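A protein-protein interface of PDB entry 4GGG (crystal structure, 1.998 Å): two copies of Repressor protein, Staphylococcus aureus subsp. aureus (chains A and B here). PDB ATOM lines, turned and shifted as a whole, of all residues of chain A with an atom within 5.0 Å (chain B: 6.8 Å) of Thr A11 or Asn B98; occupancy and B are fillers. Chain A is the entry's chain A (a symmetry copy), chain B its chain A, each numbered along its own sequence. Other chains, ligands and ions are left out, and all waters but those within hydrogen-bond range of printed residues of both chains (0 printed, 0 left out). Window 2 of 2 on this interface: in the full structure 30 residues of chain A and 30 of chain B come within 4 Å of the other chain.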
ATOM      1  N   ASP A  10      14.466  30.416   9.564  1.00  0.00           N
ATOM      2  CA  ASP A  10      15.700  30.004   8.905  1.00  0.00           C
ATOM      3  C   ASP A  10      16.151  28.611   9.333  1.00  0.00           C
ATOM      4  O   ASP A  10      16.634  27.830   8.514  1.00  0.00           O
ATOM      5  CB  ASP A  10      16.816  31.017   9.159  1.00  0.00           C
ATOM      6  CG  ASP A  10      16.905  32.066   8.071  1.00  0.00           C
ATOM      7  OD1 ASP A  10      15.983  32.127   7.228  1.00  0.00           O
ATOM      8  OD2 ASP A  10      17.892  32.833   8.058  1.00  0.00           O
ATOM      9  N   THR A  11      16.001  28.304  10.617  1.00  0.00           N
ATOM     10  CA  THR A  11      16.375  26.990  11.124  1.00  0.00           C
ATOM     11  C   THR A  11      15.648  25.899  10.349  1.00  0.00           C
ATOM     12  O   THR A  11      16.260  24.932   9.899  1.00  0.00           O
ATOM     13  CB  THR A  11      16.059  26.844  12.625  1.00  0.00           C
ATOM     14  OG1 THR A  11      17.002  27.604  13.391  1.00  0.00           O
ATOM     15  CG2 THR A  11      16.144  25.380  13.048  1.00  0.00           C
ATOM     16  N   LEU A  12      14.340  26.065  10.184  1.00  0.00           N
ATOM     17  CA  LEU A  12      13.532  25.047   9.520  1.00  0.00           C
ATOM     18  C   LEU A  12      13.752  25.036   8.005  1.00  0.00           C
ATOM     19  O   LEU A  12      13.600  24.000   7.356  1.00  0.00           O
ATOM     20  CB  LEU A  12      12.048  25.201   9.870  1.00  0.00           C
ATOM     21  CG  LEU A  12      11.750  25.117  11.370  1.00  0.00           C
ATOM     22  CD1 LEU A  12      10.262  25.183  11.631  1.00  0.00           C
ATOM     23  CD2 LEU A  12      12.332  23.841  11.957  1.00  0.00           C
ATOM     24  N   GLU A  13      14.115  26.180   7.441  1.00  0.00           N
ATOM     25  CA  GLU A  13      14.506  26.213   6.035  1.00  0.00           C
ATOM     26  C   GLU A  13      15.821  25.458   5.826  1.00  0.00           C
ATOM     27  O   GLU A  13      15.988  24.736   4.841  1.00  0.00           O
ATOM     28  CB  GLU A  13      14.602  27.652   5.524  1.00  0.00           C
ATOM     29  CG  GLU A  13      13.270  28.198   5.020  1.00  0.00           C
ATOM     30  CD  GLU A  13      13.177  29.710   5.089  1.00  0.00           C
ATOM     31  OE1 GLU A  13      13.073  30.252   6.212  1.00  0.00           O
ATOM     32  OE2 GLU A  13      13.199  30.357   4.021  1.00  0.00           O
ATOM     33  N   ARG A  14      16.750  25.618   6.760  1.00  0.00           N
ATOM     34  CA  ARG A  14      18.007  24.887   6.684  1.00  0.00           C
ATOM     35  C   ARG A  14      17.767  23.384   6.857  1.00  0.00           C
ATOM     36  O   ARG A  14      18.374  22.575   6.159  1.00  0.00           O
ATOM     37  CB  ARG A  14      19.025  25.423   7.696  1.00  0.00           C
ATOM     38  CG  ARG A  14      19.428  26.872   7.434  1.00  0.00           C
ATOM     39  CD  ARG A  14      20.669  27.293   8.220  1.00  0.00           C
ATOM     40  NE  ARG A  14      20.487  27.185   9.666  1.00  0.00           N
ATOM     41  CZ  ARG A  14      19.883  28.102  10.419  1.00  0.00           C
ATOM     42  NH1 ARG A  14      19.391  29.204   9.865  1.00  0.00           N
ATOM     43  NH2 ARG A  14      19.766  27.916  11.728  1.00  0.00           N
ATOM     44  N   VAL A  15      16.873  23.007   7.767  1.00  0.00           N
ATOM     45  CA  VAL A  15      16.538  21.591   7.929  1.00  0.00           C
ATOM     46  C   VAL A  15      15.952  21.042   6.633  1.00  0.00           C
ATOM     47  O   VAL A  15      16.278  19.927   6.212  1.00  0.00           O
ATOM     48  CB  VAL A  15      15.545  21.344   9.078  1.00  0.00           C
ATOM     49  CG1 VAL A  15      15.034  19.908   9.040  1.00  0.00           C
ATOM     50  CG2 VAL A  15      16.190  21.646  10.416  1.00  0.00           C
ATOM     51  N   TYR B  25       9.410  22.411   3.070  1.00  0.00           N
ATOM     52  CA  TYR B  25       9.361  23.360   4.175  1.00  0.00           C
ATOM     53  C   TYR B  25       8.086  23.235   5.005  1.00  0.00           C
ATOM     54  O   TYR B  25       8.142  23.181   6.231  1.00  0.00           O
ATOM     55  CB  TYR B  25       9.538  24.789   3.651  1.00  0.00           C
ATOM     56  CG  TYR B  25       9.514  25.856   4.721  1.00  0.00           C
ATOM     57  CD1 TYR B  25      10.480  25.893   5.720  1.00  0.00           C
ATOM     58  CD2 TYR B  25       8.532  26.836   4.724  1.00  0.00           C
ATOM     59  CE1 TYR B  25      10.461  26.880   6.702  1.00  0.00           C
ATOM     60  CE2 TYR B  25       8.505  27.821   5.692  1.00  0.00           C
ATOM     61  CZ  TYR B  25       9.467  27.842   6.677  1.00  0.00           C
ATOM     62  OH  TYR B  25       9.424  28.831   7.632  1.00  0.00           O
ATOM     63  N   ILE B  28       8.079  20.024   6.927  1.00  0.00           N
ATOM     64  CA  ILE B  28       8.963  20.170   8.077  1.00  0.00           C
ATOM     65  C   ILE B  28       8.278  20.977   9.188  1.00  0.00           C
ATOM     66  O   ILE B  28       8.375  20.627  10.366  1.00  0.00           O
ATOM     67  CB  ILE B  28      10.324  20.780   7.697  1.00  0.00           C
ATOM     68  CG1 ILE B  28      11.130  19.773   6.871  1.00  0.00           C
ATOM     69  CG2 ILE B  28      11.113  21.154   8.946  1.00  0.00           C
ATOM     70  CD1 ILE B  28      11.374  18.466   7.596  1.00  0.00           C
ATOM     71  N   ALA B  93      18.388  16.602  13.391  1.00  0.00           N
ATOM     72  CA  ALA B  93      18.537  17.437  12.194  1.00  0.00           C
ATOM     73  C   ALA B  93      18.403  18.922  12.531  1.00  0.00           C
ATOM     74  O   ALA B  93      19.197  19.750  12.077  1.00  0.00           O
ATOM     75  CB  ALA B  93      17.523  17.040  11.137  1.00  0.00           C
ATOM     76  N   ILE B  94      17.392  19.260  13.322  1.00  0.00           N
ATOM     77  CA  ILE B  94      17.183  20.647  13.727  1.00  0.00           C
ATOM     78  C   ILE B  94      18.400  21.182  14.469  1.00  0.00           C
ATOM     79  O   ILE B  94      18.864  22.300  14.212  1.00  0.00           O
ATOM     80  CB  ILE B  94      15.918  20.807  14.604  1.00  0.00           C
ATOM     81  CG1 ILE B  94      14.663  20.598  13.747  1.00  0.00           C
ATOM     82  CG2 ILE B  94      15.885  22.191  15.252  1.00  0.00           C
ATOM     83  CD1 ILE B  94      13.350  20.584  14.536  1.00  0.00           C
ATOM     84  N   HIS B  95      18.917  20.364  15.382  1.00  0.00           N
ATOM     85  CA  HIS B  95      20.091  20.722  16.156  1.00  0.00           C
ATOM     86  C   HIS B  95      21.288  20.910  15.223  1.00  0.00           C
ATOM     87  O   HIS B  95      22.069  21.848  15.368  1.00  0.00           O
ATOM     88  CB  HIS B  95      20.380  19.614  17.174  1.00  0.00           C
ATOM     89  CG  HIS B  95      21.652  19.806  17.936  1.00  0.00           C
ATOM     90  ND1 HIS B  95      21.849  20.855  18.807  1.00  0.00           N
ATOM     91  CD2 HIS B  95      22.790  19.073  17.965  1.00  0.00           C
ATOM     92  CE1 HIS B  95      23.057  20.765  19.335  1.00  0.00           C
ATOM     93  NE2 HIS B  95      23.647  19.690  18.844  1.00  0.00           N
ATOM     94  N   HIS B  96      21.424  20.011  14.260  1.00  0.00           N
ATOM     95  CA  HIS B  96      22.549  20.070  13.332  1.00  0.00           C
ATOM     96  C   HIS B  96      22.503  21.369  12.530  1.00  0.00           C
ATOM     97  O   HIS B  96      23.533  21.994  12.276  1.00  0.00           O
ATOM     98  CB  HIS B  96      22.533  18.864  12.391  1.00  0.00           C
ATOM     99  CG  HIS B  96      23.710  18.802  11.466  1.00  0.00           C
ATOM    100  ND1 HIS B  96      24.998  18.598  11.912  1.00  0.00           N
ATOM    101  CD2 HIS B  96      23.793  18.922  10.121  1.00  0.00           C
ATOM    102  CE1 HIS B  96      25.824  18.585  10.880  1.00  0.00           C
ATOM    103  NE2 HIS B  96      25.116  18.782   9.782  1.00  0.00           N
ATOM    104  N   ALA B  97      21.298  21.769  12.139  1.00  0.00           N
ATOM    105  CA  ALA B  97      21.098  22.989  11.375  1.00  0.00           C
ATOM    106  C   ALA B  97      21.452  24.226  12.189  1.00  0.00           C
ATOM    107  O   ALA B  97      21.861  25.244  11.634  1.00  0.00           O
ATOM    108  CB  ALA B  97      19.652  23.074  10.899  1.00  0.00           C
ATOM    109  N   ASN B  98      21.297  24.133  13.508  1.00  0.00           N
ATOM    110  CA  ASN B  98      21.512  25.272  14.392  1.00  0.00           C
ATOM    111  C   ASN B  98      22.957  25.555  14.774  1.00  0.00           C
ATOM    112  O   ASN B  98      23.359  26.712  14.849  1.00  0.00           O
ATOM    113  CB  ASN B  98      20.670  25.137  15.664  1.00  0.00           C
ATOM    114  CG  ASN B  98      19.281  25.717  15.506  1.00  0.00           C
ATOM    115  OD1 ASN B  98      19.052  26.580  14.659  1.00  0.00           O
ATOM    116  ND2 ASN B  98      18.347  25.253  16.327  1.00  0.00           N
ATOM    117  N   HIS B  99      23.740  24.513  15.028  1.00  0.00           N
ATOM    118  CA  HIS B  99      25.089  24.738  15.543  1.00  0.00           C
ATOM    119  C   HIS B  99      26.032  25.295  14.473  1.00  0.00           C
ATOM    120  O   HIS B  99      25.766  25.168  13.276  1.00  0.00           O
ATOM    121  CB  HIS B  99      25.652  23.487  16.242  1.00  0.00           C
ATOM    122  CG  HIS B  99      25.973  22.354  15.319  1.00  0.00           C
ATOM    123  ND1 HIS B  99      26.891  22.460  14.297  1.00  0.00           N
ATOM    124  CD2 HIS B  99      25.520  21.078  15.287  1.00  0.00           C
ATOM    125  CE1 HIS B  99      26.983  21.301  13.668  1.00  0.00           C
ATOM    126  NE2 HIS B  99      26.159  20.447  14.246  1.00  0.00           N
ATOM    127  N   PRO B 100      27.119  25.951  14.906  1.00  0.00           N
ATOM    128  CA  PRO B 100      28.096  26.549  13.988  1.00  0.00           C
ATOM    129  C   PRO B 100      28.787  25.509  13.104  1.00  0.00           C
ATOM    130  O   PRO B 100      29.025  24.383  13.542  1.00  0.00           O
ATOM    131  CB  PRO B 100      29.111  27.199  14.935  1.00  0.00           C
ATOM    132  CG  PRO B 100      28.353  27.434  16.198  1.00  0.00           C
ATOM    133  CD  PRO B 100      27.421  26.271  16.312  1.00  0.00           C
ATOM    134  N   LYS B 101      29.108  25.894  11.872  1.00  0.00           N
ATOM    135  CA  LYS B 101      29.736  24.985  10.919  1.00  0.00           C
ATOM    136  C   LYS B 101      31.205  25.337  10.701  1.00  0.00           C
ATOM    137  O   LYS B 101      31.604  25.743   9.608  1.00  0.00           O
ATOM    138  CB  LYS B 101      28.987  25.018   9.587  1.00  0.00           C
ATOM    139  CG  LYS B 101      27.476  24.882   9.718  1.00  0.00           C
ATOM    140  CD  LYS B 101      27.071  23.510  10.226  1.00  0.00           C
ATOM    141  CE  LYS B 101      25.560  23.392  10.303  1.00  0.00           C
ATOM    142  NZ  LYS B 101      25.113  22.008   9.999  1.00  0.00           N
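The side-chain amide oxygen of Asn B98 is in hydrogen-bond range of the side-chain hydroxyl of Thr A11 (2.6 Å).
NH2 of Arg A14 lies within hydrogen-bond range of OD1 of Asn B98, 3.3 Å away.
NE of Arg A14 sits at hydrogen-bond distance from O of Ala B97, 3.1 Å away.
The side-chain hydroxyl (OG1) of Thr A11 sits at hydrogen-bond distance from the guanidinium group (NH2) of Arg A14 (3.2 Å).
The guanidinium group (NH1) of Arg A14 sits close to the backbone carbonyl oxygen (O) of Asp A10 (3.4 Å).
Thr A11 touches Ile B94.
O of Thr A11 touches CB of Ala B97, at 3.99 Å.
Tyr B25 touches Leu A12.
Glu A13 touches Tyr B25 (CG to CE1, 3.5 Å).
Val A15 touches Ala B93 (CG2 to O, 3.9 Å).
Ile B94 touches Val A15.
Val A15 touches Ala B97.
Of the printed residues of chain B, Thr A11 touches Ile B94 (3.9 Å), Ala B97 (3.99 Å) and Asn B98 (2.6 Å).
Of chain A, only Thr A11 and Arg A14 come within 4 Å of Asn B98.
Of the printed residues of chain A, Tyr B25 touches Leu A12 (3.9 Å) and Glu A13 (3.5 Å).
Of the printed residues of chain B, Glu A13 touches Tyr B25 (3.5 Å).
Of the printed residues of chain B, Leu A12 touches Tyr B25 (3.9 Å).
Printed residues of chain A within 4 Å of Ile B94: Thr A11 and Val A15.
Printed residues of chain A within 4 Å of Ala B93: Val A15 (3.9 Å).
His B95 touches none of the printed residues of chain A.
His B99 touches none of the printed residues of chain A.
The nearest printed residue of chain B that does not touch Thr A11 is His B95 (6.2 Å).
The nearest printed residue of chain A that does not touch Ala B93 is Thr A11 (6.3 Å).
Hydrophobic or aromatic side chains of chain A within 4 Å of the printed part of chain B: Leu A12 and Val A15.
Along chain A the printed residues that touch a printed residue of chain B span positions 11 to 15.
Along chain B the printed residues that touch a printed residue of chain A span positions 25 to 98.
Among the printed residues, no Asp or Glu carboxylate lies within 4 Å of a Lys or Arg side-chain nitrogen of the other chain.
No position is printed for both chains.
Of the 10 pairs that touch across the chains among the printed residues, none has its exchanged pair printed and touching as well.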
